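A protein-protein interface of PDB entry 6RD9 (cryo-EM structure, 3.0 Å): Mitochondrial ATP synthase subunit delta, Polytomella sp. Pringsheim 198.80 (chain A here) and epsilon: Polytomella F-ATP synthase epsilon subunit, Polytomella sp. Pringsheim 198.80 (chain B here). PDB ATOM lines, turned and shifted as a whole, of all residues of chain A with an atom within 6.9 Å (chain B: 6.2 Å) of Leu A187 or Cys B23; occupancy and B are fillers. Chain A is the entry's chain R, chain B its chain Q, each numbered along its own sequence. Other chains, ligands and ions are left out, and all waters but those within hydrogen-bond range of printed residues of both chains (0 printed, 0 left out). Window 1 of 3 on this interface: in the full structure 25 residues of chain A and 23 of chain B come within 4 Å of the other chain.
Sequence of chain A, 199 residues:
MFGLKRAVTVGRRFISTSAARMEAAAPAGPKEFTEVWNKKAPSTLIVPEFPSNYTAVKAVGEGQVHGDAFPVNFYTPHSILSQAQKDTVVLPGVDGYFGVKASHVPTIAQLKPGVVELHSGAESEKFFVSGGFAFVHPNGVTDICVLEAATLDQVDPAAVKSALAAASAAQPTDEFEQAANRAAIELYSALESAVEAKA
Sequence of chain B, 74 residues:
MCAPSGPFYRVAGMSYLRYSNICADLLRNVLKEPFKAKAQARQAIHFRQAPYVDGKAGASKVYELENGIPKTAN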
ATOM      1  N   PRO A 113     -21.127  -9.346   4.605  1.00  0.00           N
ATOM      2  CA  PRO A 113     -21.642  -8.607   3.452  1.00  0.00           C
ATOM      3  C   PRO A 113     -23.151  -8.486   3.498  1.00  0.00           C
ATOM      4  O   PRO A 113     -23.861  -9.479   3.346  1.00  0.00           O
ATOM      5  CB  PRO A 113     -21.187  -9.461   2.270  1.00  0.00           C
ATOM      6  CG  PRO A 113     -19.955 -10.092   2.738  1.00  0.00           C
ATOM      7  CD  PRO A 113     -20.102 -10.323   4.203  1.00  0.00           C
ATOM      8  N   GLY A 114     -23.651  -7.284   3.721  1.00  0.00           N
ATOM      9  CA  GLY A 114     -25.079  -7.104   3.846  1.00  0.00           C
ATOM     10  C   GLY A 114     -25.429  -5.642   3.776  1.00  0.00           C
ATOM     11  O   GLY A 114     -24.581  -4.800   3.499  1.00  0.00           O
ATOM     12  N   PHE A 128     -25.366  -1.153   0.878  1.00  0.00           N
ATOM     13  CA  PHE A 128     -24.856  -2.514   0.932  1.00  0.00           C
ATOM     14  C   PHE A 128     -23.352  -2.467   1.145  1.00  0.00           C
ATOM     15  O   PHE A 128     -22.635  -1.842   0.360  1.00  0.00           O
ATOM     16  CB  PHE A 128     -25.180  -3.264  -0.356  1.00  0.00           C
ATOM     17  CG  PHE A 128     -24.671  -4.669  -0.385  1.00  0.00           C
ATOM     18  CD1 PHE A 128     -25.353  -5.677   0.262  1.00  0.00           C
ATOM     19  CD2 PHE A 128     -23.516  -4.986  -1.071  1.00  0.00           C
ATOM     20  CE1 PHE A 128     -24.887  -6.970   0.233  1.00  0.00           C
ATOM     21  CE2 PHE A 128     -23.045  -6.274  -1.103  1.00  0.00           C
ATOM     22  CZ  PHE A 128     -23.732  -7.269  -0.452  1.00  0.00           C
ATOM     23  N   VAL A 129     -22.869  -3.135   2.190  1.00  0.00           N
ATOM     24  CA  VAL A 129     -21.457  -3.077   2.544  1.00  0.00           C
ATOM     25  C   VAL A 129     -20.824  -4.444   2.356  1.00  0.00           C
ATOM     26  O   VAL A 129     -21.499  -5.463   2.238  1.00  0.00           O
ATOM     27  CB  VAL A 129     -21.242  -2.577   3.974  1.00  0.00           C
ATOM     28  CG1 VAL A 129     -21.868  -1.232   4.132  1.00  0.00           C
ATOM     29  CG2 VAL A 129     -21.818  -3.543   4.956  1.00  0.00           C
ATOM     30  N   SER A 130     -19.503  -4.452   2.324  1.00  0.00           N
ATOM     31  CA  SER A 130     -18.749  -5.649   1.993  1.00  0.00           C
ATOM     32  C   SER A 130     -18.347  -6.459   3.210  1.00  0.00           C
ATOM     33  O   SER A 130     -17.722  -7.511   3.056  1.00  0.00           O
ATOM     34  CB  SER A 130     -17.490  -5.274   1.225  1.00  0.00           C
ATOM     35  OG  SER A 130     -16.600  -4.576   2.073  1.00  0.00           O
ATOM     36  N   GLY A 131     -18.687  -6.012   4.401  1.00  0.00           N
ATOM     37  CA  GLY A 131     -18.144  -6.653   5.577  1.00  0.00           C
ATOM     38  C   GLY A 131     -17.190  -5.679   6.230  1.00  0.00           C
ATOM     39  O   GLY A 131     -16.626  -4.798   5.575  1.00  0.00           O
ATOM     40  N   LEU A 147     -15.354  -1.390   4.299  1.00  0.00           N
ATOM     41  CA  LEU A 147     -14.417  -1.051   3.238  1.00  0.00           C
ATOM     42  C   LEU A 147     -15.112  -0.467   2.016  1.00  0.00           C
ATOM     43  O   LEU A 147     -14.903   0.699   1.682  1.00  0.00           O
ATOM     44  CB  LEU A 147     -13.599  -2.274   2.829  1.00  0.00           C
ATOM     45  CG  LEU A 147     -12.206  -2.272   3.435  1.00  0.00           C
ATOM     46  CD1 LEU A 147     -12.283  -2.499   4.894  1.00  0.00           C
ATOM     47  CD2 LEU A 147     -11.354  -3.317   2.788  1.00  0.00           C
ATOM     48  N   GLU A 148     -15.953  -1.246   1.357  1.00  0.00           N
ATOM     49  CA  GLU A 148     -16.705  -0.772   0.207  1.00  0.00           C
ATOM     50  C   GLU A 148     -18.168  -0.728   0.594  1.00  0.00           C
ATOM     51  O   GLU A 148     -18.759  -1.766   0.897  1.00  0.00           O
ATOM     52  CB  GLU A 148     -16.488  -1.670  -1.004  1.00  0.00           C
ATOM     53  CG  GLU A 148     -16.878  -1.017  -2.311  1.00  0.00           C
ATOM     54  CD  GLU A 148     -15.893   0.052  -2.760  1.00  0.00           C
ATOM     55  OE1 GLU A 148     -14.712  -0.001  -2.359  1.00  0.00           O
ATOM     56  OE2 GLU A 148     -16.297   0.946  -3.531  1.00  0.00           O
ATOM     57  N   VAL A 160     -24.383  -9.663 -11.061  1.00  0.00           N
ATOM     58  CA  VAL A 160     -24.154 -10.259  -9.753  1.00  0.00           C
ATOM     59  C   VAL A 160     -24.233 -11.781  -9.827  1.00  0.00           C
ATOM     60  O   VAL A 160     -23.366 -12.479  -9.294  1.00  0.00           O
ATOM     61  CB  VAL A 160     -25.118  -9.647  -8.710  1.00  0.00           C
ATOM     62  CG1 VAL A 160     -26.575  -9.689  -9.152  1.00  0.00           C
ATOM     63  CG2 VAL A 160     -24.937 -10.308  -7.349  1.00  0.00           C
ATOM     64  N   LEU A 164     -21.659 -15.004  -9.835  1.00  0.00           N
ATOM     65  CA  LEU A 164     -22.028 -15.968  -8.804  1.00  0.00           C
ATOM     66  C   LEU A 164     -22.164 -17.367  -9.382  1.00  0.00           C
ATOM     67  O   LEU A 164     -21.820 -18.348  -8.714  1.00  0.00           O
ATOM     68  CB  LEU A 164     -23.332 -15.547  -8.130  1.00  0.00           C
ATOM     69  CG  LEU A 164     -23.840 -16.420  -6.985  1.00  0.00           C
ATOM     70  CD1 LEU A 164     -22.757 -16.667  -5.932  1.00  0.00           C
ATOM     71  CD2 LEU A 164     -25.059 -15.800  -6.362  1.00  0.00           C
ATOM     72  N   ALA A 180     -11.455 -17.746  -0.479  1.00  0.00           N
ATOM     73  CA  ALA A 180     -11.749 -16.627  -1.370  1.00  0.00           C
ATOM     74  C   ALA A 180     -12.953 -16.915  -2.252  1.00  0.00           C
ATOM     75  O   ALA A 180     -13.659 -15.991  -2.669  1.00  0.00           O
ATOM     76  CB  ALA A 180     -10.533 -16.297  -2.229  1.00  0.00           C
ATOM     77  N   ASN A 181     -13.196 -18.183  -2.563  1.00  0.00           N
ATOM     78  CA  ASN A 181     -14.430 -18.495  -3.262  1.00  0.00           C
ATOM     79  C   ASN A 181     -15.599 -18.519  -2.291  1.00  0.00           C
ATOM     80  O   ASN A 181     -16.714 -18.134  -2.660  1.00  0.00           O
ATOM     81  CB  ASN A 181     -14.303 -19.826  -3.989  1.00  0.00           C
ATOM     82  CG  ASN A 181     -15.274 -19.962  -5.127  1.00  0.00           C
ATOM     83  OD1 ASN A 181     -16.466 -19.738  -4.983  1.00  0.00           O
ATOM     84  ND2 ASN A 181     -14.756 -20.335  -6.284  1.00  0.00           N
ATOM     85  N   ARG A 182     -15.359 -18.946  -1.045  1.00  0.00           N
ATOM     86  CA  ARG A 182     -16.397 -18.887  -0.019  1.00  0.00           C
ATOM     87  C   ARG A 182     -16.819 -17.449   0.242  1.00  0.00           C
ATOM     88  O   ARG A 182     -18.013 -17.152   0.363  1.00  0.00           O
ATOM     89  CB  ARG A 182     -15.900 -19.540   1.271  1.00  0.00           C
ATOM     90  CG  ARG A 182     -16.814 -19.324   2.465  1.00  0.00           C
ATOM     91  CD  ARG A 182     -16.552 -20.328   3.564  1.00  0.00           C
ATOM     92  NE  ARG A 182     -17.240 -19.969   4.799  1.00  0.00           N
ATOM     93  CZ  ARG A 182     -17.189 -20.687   5.914  1.00  0.00           C
ATOM     94  NH1 ARG A 182     -16.479 -21.801   5.950  1.00  0.00           N
ATOM     95  NH2 ARG A 182     -17.842 -20.289   6.994  1.00  0.00           N
ATOM     96  N   ALA A 183     -15.846 -16.537   0.281  1.00  0.00           N
ATOM     97  CA  ALA A 183     -16.155 -15.120   0.403  1.00  0.00           C
ATOM     98  C   ALA A 183     -16.826 -14.592  -0.853  1.00  0.00           C
ATOM     99  O   ALA A 183     -17.632 -13.658  -0.788  1.00  0.00           O
ATOM    100  CB  ALA A 183     -14.880 -14.342   0.696  1.00  0.00           C
ATOM    101  N   ALA A 184     -16.515 -15.185  -2.005  1.00  0.00           N
ATOM    102  CA  ALA A 184     -17.154 -14.774  -3.248  1.00  0.00           C
ATOM    103  C   ALA A 184     -18.612 -15.201  -3.282  1.00  0.00           C
ATOM    104  O   ALA A 184     -19.475 -14.468  -3.776  1.00  0.00           O
ATOM    105  CB  ALA A 184     -16.401 -15.353  -4.442  1.00  0.00           C
ATOM    106  N   ILE A 185     -18.905 -16.390  -2.762  1.00  0.00           N
ATOM    107  CA  ILE A 185     -20.265 -16.910  -2.840  1.00  0.00           C
ATOM    108  C   ILE A 185     -21.180 -16.184  -1.862  1.00  0.00           C
ATOM    109  O   ILE A 185     -22.278 -15.753  -2.232  1.00  0.00           O
ATOM    110  CB  ILE A 185     -20.269 -18.433  -2.615  1.00  0.00           C
ATOM    111  CG1 ILE A 185     -19.572 -19.142  -3.772  1.00  0.00           C
ATOM    112  CG2 ILE A 185     -21.667 -18.956  -2.535  1.00  0.00           C
ATOM    113  CD1 ILE A 185     -19.308 -20.608  -3.516  1.00  0.00           C
ATOM    114  N   GLU A 186     -20.732 -15.999  -0.616  1.00  0.00           N
ATOM    115  CA  GLU A 186     -21.614 -15.448   0.411  1.00  0.00           C
ATOM    116  C   GLU A 186     -21.869 -13.963   0.190  1.00  0.00           C
ATOM    117  O   GLU A 186     -22.855 -13.414   0.693  1.00  0.00           O
ATOM    118  CB  GLU A 186     -21.030 -15.683   1.804  1.00  0.00           C
ATOM    119  CG  GLU A 186     -19.848 -14.788   2.158  1.00  0.00           C
ATOM    120  CD  GLU A 186     -19.308 -15.032   3.555  1.00  0.00           C
ATOM    121  OE1 GLU A 186     -19.765 -15.985   4.219  1.00  0.00           O
ATOM    122  OE2 GLU A 186     -18.429 -14.260   3.990  1.00  0.00           O
ATOM    123  N   LEU A 187     -20.996 -13.297  -0.565  1.00  0.00           N
ATOM    124  CA  LEU A 187     -21.193 -11.883  -0.841  1.00  0.00           C
ATOM    125  C   LEU A 187     -22.268 -11.682  -1.895  1.00  0.00           C
ATOM    126  O   LEU A 187     -23.178 -10.864  -1.710  1.00  0.00           O
ATOM    127  CB  LEU A 187     -19.868 -11.258  -1.267  1.00  0.00           C
ATOM    128  CG  LEU A 187     -19.748  -9.916  -1.981  1.00  0.00           C
ATOM    129  CD1 LEU A 187     -20.481  -8.785  -1.315  1.00  0.00           C
ATOM    130  CD2 LEU A 187     -18.297  -9.591  -1.993  1.00  0.00           C
ATOM    131  N   TYR A 188     -22.188 -12.421  -2.999  1.00  0.00           N
ATOM    132  CA  TYR A 188     -23.181 -12.266  -4.050  1.00  0.00           C
ATOM    133  C   TYR A 188     -24.525 -12.832  -3.626  1.00  0.00           C
ATOM    134  O   TYR A 188     -25.564 -12.318  -4.043  1.00  0.00           O
ATOM    135  CB  TYR A 188     -22.710 -12.951  -5.326  1.00  0.00           C
ATOM    136  CG  TYR A 188     -21.470 -12.347  -5.911  1.00  0.00           C
ATOM    137  CD1 TYR A 188     -21.240 -10.982  -5.841  1.00  0.00           C
ATOM    138  CD2 TYR A 188     -20.513 -13.147  -6.514  1.00  0.00           C
ATOM    139  CE1 TYR A 188     -20.093 -10.435  -6.360  1.00  0.00           C
ATOM    140  CE2 TYR A 188     -19.364 -12.605  -7.041  1.00  0.00           C
ATOM    141  CZ  TYR A 188     -19.161 -11.249  -6.964  1.00  0.00           C
ATOM    142  OH  TYR A 188     -18.017 -10.706  -7.494  1.00  0.00           O
ATOM    143  N   SER A 189     -24.519 -13.870  -2.783  1.00  0.00           N
ATOM    144  CA  SER A 189     -25.760 -14.493  -2.341  1.00  0.00           C
ATOM    145  C   SER A 189     -26.564 -13.557  -1.455  1.00  0.00           C
ATOM    146  O   SER A 189     -27.793 -13.496  -1.560  1.00  0.00           O
ATOM    147  CB  SER A 189     -25.452 -15.771  -1.584  1.00  0.00           C
ATOM    148  OG  SER A 189     -24.507 -16.546  -2.296  1.00  0.00           O
ATOM    149  N   ALA A 190     -25.887 -12.827  -0.572  1.00  0.00           N
ATOM    150  CA  ALA A 190     -26.564 -11.773   0.166  1.00  0.00           C
ATOM    151  C   ALA A 190     -26.893 -10.603  -0.746  1.00  0.00           C
ATOM    152  O   ALA A 190     -27.854  -9.867  -0.501  1.00  0.00           O
ATOM    153  CB  ALA A 190     -25.702 -11.315   1.335  1.00  0.00           C
ATOM    154  N   LEU A 191     -26.100 -10.419  -1.803  1.00  0.00           N
ATOM    155  CA  LEU A 191     -26.388  -9.368  -2.765  1.00  0.00           C
ATOM    156  C   LEU A 191     -27.547  -9.749  -3.671  1.00  0.00           C
ATOM    157  O   LEU A 191     -28.275  -8.863  -4.125  1.00  0.00           O
ATOM    158  CB  LEU A 191     -25.139  -9.052  -3.586  1.00  0.00           C
ATOM    159  CG  LEU A 191     -25.096  -7.764  -4.404  1.00  0.00           C
ATOM    160  CD1 LEU A 191     -25.646  -6.597  -3.616  1.00  0.00           C
ATOM    161  CD2 LEU A 191     -23.674  -7.490  -4.824  1.00  0.00           C
ATOM    162  N   GLU A 192     -27.735 -11.046  -3.944  1.00  0.00           N
ATOM    163  CA  GLU A 192     -28.921 -11.487  -4.677  1.00  0.00           C
ATOM    164  C   GLU A 192     -30.184 -11.170  -3.899  1.00  0.00           C
ATOM    165  O   GLU A 192     -31.105 -10.536  -4.419  1.00  0.00           O
ATOM    166  CB  GLU A 192     -28.871 -12.990  -4.958  1.00  0.00           C
ATOM    167  CG  GLU A 192     -27.847 -13.455  -5.959  1.00  0.00           C
ATOM    168  CD  GLU A 192     -28.099 -12.952  -7.351  1.00  0.00           C
ATOM    169  OE1 GLU A 192     -29.273 -12.782  -7.734  1.00  0.00           O
ATOM    170  OE2 GLU A 192     -27.107 -12.724  -8.063  1.00  0.00           O
ATOM    171  N   ARG B  18      -6.615  -9.073   3.800  1.00  0.00           N
ATOM    172  CA  ARG B  18      -6.776  -9.586   2.452  1.00  0.00           C
ATOM    173  C   ARG B  18      -8.202 -10.030   2.211  1.00  0.00           C
ATOM    174  O   ARG B  18      -8.760  -9.754   1.150  1.00  0.00           O
ATOM    175  CB  ARG B  18      -5.821 -10.739   2.192  1.00  0.00           C
ATOM    176  CG  ARG B  18      -5.738 -11.063   0.725  1.00  0.00           C
ATOM    177  CD  ARG B  18      -4.721 -12.120   0.457  1.00  0.00           C
ATOM    178  NE  ARG B  18      -3.374 -11.607   0.615  1.00  0.00           N
ATOM    179  CZ  ARG B  18      -2.629 -11.189  -0.395  1.00  0.00           C
ATOM    180  NH1 ARG B  18      -3.108 -11.220  -1.630  1.00  0.00           N
ATOM    181  NH2 ARG B  18      -1.408 -10.740  -0.168  1.00  0.00           N
ATOM    182  N   TYR B  19      -8.813 -10.671   3.206  1.00  0.00           N
ATOM    183  CA  TYR B  19     -10.182 -11.150   3.072  1.00  0.00           C
ATOM    184  C   TYR B  19     -11.153  -9.994   2.919  1.00  0.00           C
ATOM    185  O   TYR B  19     -12.065 -10.038   2.088  1.00  0.00           O
ATOM    186  CB  TYR B  19     -10.553 -12.003   4.284  1.00  0.00           C
ATOM    187  CG  TYR B  19     -12.034 -12.074   4.539  1.00  0.00           C
ATOM    188  CD1 TYR B  19     -12.607 -11.393   5.601  1.00  0.00           C
ATOM    189  CD2 TYR B  19     -12.859 -12.818   3.716  1.00  0.00           C
ATOM    190  CE1 TYR B  19     -13.951 -11.443   5.824  1.00  0.00           C
ATOM    191  CE2 TYR B  19     -14.202 -12.873   3.937  1.00  0.00           C
ATOM    192  CZ  TYR B  19     -14.745 -12.185   4.992  1.00  0.00           C
ATOM    193  OH  TYR B  19     -16.099 -12.243   5.220  1.00  0.00           O
ATOM    194  N   SER B  20     -10.967  -8.944   3.708  1.00  0.00           N
ATOM    195  CA  SER B  20     -11.912  -7.846   3.670  1.00  0.00           C
ATOM    196  C   SER B  20     -11.726  -6.999   2.426  1.00  0.00           C
ATOM    197  O   SER B  20     -12.648  -6.283   2.029  1.00  0.00           O
ATOM    198  CB  SER B  20     -11.771  -7.001   4.922  1.00  0.00           C
ATOM    199  OG  SER B  20     -12.390  -5.754   4.735  1.00  0.00           O
ATOM    200  N   ASN B  21     -10.553  -7.073   1.798  1.00  0.00           N
ATOM    201  CA  ASN B  21     -10.336  -6.380   0.535  1.00  0.00           C
ATOM    202  C   ASN B  21     -10.779  -7.199  -0.665  1.00  0.00           C
ATOM    203  O   ASN B  21     -11.150  -6.614  -1.685  1.00  0.00           O
ATOM    204  CB  ASN B  21      -8.870  -5.993   0.383  1.00  0.00           C
ATOM    205  CG  ASN B  21      -8.588  -4.625   0.923  1.00  0.00           C
ATOM    206  OD1 ASN B  21      -8.876  -3.630   0.274  1.00  0.00           O
ATOM    207  ND2 ASN B  21      -8.018  -4.559   2.111  1.00  0.00           N
ATOM    208  N   ILE B  22     -10.718  -8.532  -0.582  1.00  0.00           N
ATOM    209  CA  ILE B  22     -11.332  -9.368  -1.612  1.00  0.00           C
ATOM    210  C   ILE B  22     -12.829  -9.112  -1.668  1.00  0.00           C
ATOM    211  O   ILE B  22     -13.390  -8.866  -2.738  1.00  0.00           O
ATOM    212  CB  ILE B  22     -11.024 -10.857  -1.376  1.00  0.00           C
ATOM    213  CG1 ILE B  22      -9.543 -11.156  -1.568  1.00  0.00           C
ATOM    214  CG2 ILE B  22     -11.821 -11.715  -2.308  1.00  0.00           C
ATOM    215  CD1 ILE B  22      -9.155 -12.540  -1.143  1.00  0.00           C
ATOM    216  N   CYS B  23     -13.482  -9.093  -0.508  1.00  0.00           N
ATOM    217  CA  CYS B  23     -14.900  -8.758  -0.456  1.00  0.00           C
ATOM    218  C   CYS B  23     -15.159  -7.309  -0.842  1.00  0.00           C
ATOM    219  O   CYS B  23     -16.259  -6.979  -1.284  1.00  0.00           O
ATOM    220  CB  CYS B  23     -15.457  -9.036   0.936  1.00  0.00           C
ATOM    221  SG  CYS B  23     -15.468 -10.771   1.357  1.00  0.00           S
ATOM    222  N   ALA B  24     -14.171  -6.434  -0.682  1.00  0.00           N
ATOM    223  CA  ALA B  24     -14.308  -5.088  -1.217  1.00  0.00           C
ATOM    224  C   ALA B  24     -14.130  -5.081  -2.727  1.00  0.00           C
ATOM    225  O   ALA B  24     -14.777  -4.295  -3.427  1.00  0.00           O
ATOM    226  CB  ALA B  24     -13.305  -4.156  -0.552  1.00  0.00           C
ATOM    227  N   ASP B  25     -13.265  -5.960  -3.243  1.00  0.00           N
ATOM    228  CA  ASP B  25     -13.016  -6.031  -4.680  1.00  0.00           C
ATOM    229  C   ASP B  25     -14.234  -6.555  -5.421  1.00  0.00           C
ATOM    230  O   ASP B  25     -14.611  -6.032  -6.476  1.00  0.00           O
ATOM    231  CB  ASP B  25     -11.820  -6.934  -4.966  1.00  0.00           C
ATOM    232  CG  ASP B  25     -10.500  -6.219  -4.838  1.00  0.00           C
ATOM    233  OD1 ASP B  25     -10.495  -4.984  -4.656  1.00  0.00           O
ATOM    234  OD2 ASP B  25      -9.459  -6.896  -4.938  1.00  0.00           O
ATOM    235  N   LEU B  26     -14.861  -7.598  -4.880  1.00  0.00           N
ATOM    236  CA  LEU B  26     -15.962  -8.242  -5.576  1.00  0.00           C
ATOM    237  C   LEU B  26     -17.226  -7.405  -5.543  1.00  0.00           C
ATOM    238  O   LEU B  26     -18.092  -7.577  -6.403  1.00  0.00           O
ATOM    239  CB  LEU B  26     -16.207  -9.618  -4.978  1.00  0.00           C
ATOM    240  CG  LEU B  26     -14.971 -10.504  -5.000  1.00  0.00           C
ATOM    241  CD1 LEU B  26     -15.235 -11.799  -4.303  1.00  0.00           C
ATOM    242  CD2 LEU B  26     -14.547 -10.746  -6.432  1.00  0.00           C
ATOM    243  N   LEU B  27     -17.357  -6.500  -4.576  1.00  0.00           N
ATOM    244  CA  LEU B  27     -18.469  -5.564  -4.636  1.00  0.00           C
ATOM    245  C   LEU B  27     -18.290  -4.566  -5.772  1.00  0.00           C
ATOM    246  O   LEU B  27     -19.271  -4.198  -6.419  1.00  0.00           O
ATOM    247  CB  LEU B  27     -18.626  -4.842  -3.300  1.00  0.00           C
ATOM    248  CG  LEU B  27     -19.761  -3.830  -3.130  1.00  0.00           C
ATOM    249  CD1 LEU B  27     -21.067  -4.359  -3.654  1.00  0.00           C
ATOM    250  CD2 LEU B  27     -19.927  -3.503  -1.679  1.00  0.00           C
ATOM    251  N   ARG B  28     -17.053  -4.153  -6.058  1.00  0.00           N
ATOM    252  CA  ARG B  28     -16.830  -3.127  -7.073  1.00  0.00           C
ATOM    253  C   ARG B  28     -17.087  -3.645  -8.482  1.00  0.00           C
ATOM    254  O   ARG B  28     -17.476  -2.868  -9.358  1.00  0.00           O
ATOM    255  CB  ARG B  28     -15.407  -2.581  -6.971  1.00  0.00           C
ATOM    256  CG  ARG B  28     -15.103  -1.885  -5.661  1.00  0.00           C
ATOM    257  CD  ARG B  28     -13.723  -1.274  -5.674  1.00  0.00           C
ATOM    258  NE  ARG B  28     -13.272  -0.960  -4.327  1.00  0.00           N
ATOM    259  CZ  ARG B  28     -12.366  -1.667  -3.672  1.00  0.00           C
ATOM    260  NH1 ARG B  28     -11.809  -2.719  -4.252  1.00  0.00           N
ATOM    261  NH2 ARG B  28     -12.017  -1.322  -2.444  1.00  0.00           N
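The side-chain hydroxyl (OH) of Tyr B19 lies within hydrogen-bond range of the side-chain carboxylate (OE2) of Glu A186 (3.3 Å). The side-chain hydroxyl of Tyr A188 sits close to the backbone carbonyl oxygen of Leu B26 (3.3 Å). The guanidinium group (NE) of Arg B28 is in salt-bridge range of the side-chain carboxylate (OE1) of Glu A148 (2.6 Å).
The side-chain sulfur (SG) of Cys B23 is in hydrogen-bond range of the backbone carbonyl oxygen (O) of Tyr B19. The backbone carbonyl oxygen (O) of Ala B24 lies close to the guanidinium group (NH1) of Arg B28. OD1 of Asp B25 lies within salt-bridge range of NH1 of Arg B28, 2.6 Å away. The backbone NH of Ser A130 lies within hydrogen-bond range of the backbone carbonyl oxygen of Glu A148 (3.1 Å).
Among the printed residues, pairs that only touch across the chains: Phe A128 with Leu B27, Ser A130 with Cys B23, Ser A130 with Ala B24, Leu A147 with Ser B20, Leu A147 with Asn B21, Leu A147 with Ala B24, Glu A148 with Ala B24, Glu A148 with Leu B27, Ala A183 with Tyr B19, Ala A183 with Cys B23, Ala A184 with Leu B26, Leu A187 with Cys B23 and Leu A187 with Leu B26.
Printed residues of chain B within 4 Å of Ala A183: Tyr B19 and Cys B23. Leu A187 touches just these residues of chain B: Cys B23 (3.4 Å) and Leu B26 (3.6 Å). Of chain A, only Ser A130, Ala A183 and Leu A187 come within 4 Å of Cys B23. Of the printed residues of chain A, Leu B26 touches Ala A184, Leu A187 and Tyr A188. The nearest residue of chain A that does not touch Cys B23 is Pro A113 (4.7 Å). The nearest printed residue of chain B that does not touch Ala A183 is Leu B26 (4.6 Å).
Of the 23 printed residues of chain A, 9 touch a printed residue of chain B. Hydrophobic or aromatic side chains of chain A within 4 Å of the printed part of chain B: Phe A128, Leu A147, Ala A183, Ala A184, Leu A187 and Tyr A188. Printed residues of chain B that touch a printed residue of chain A: Tyr B19, Ser B20, Asn B21, Cys B23, Ala B24, Leu B26, Leu B27 and Arg B28. Among the printed residues, 16 pairs touch across the chains.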
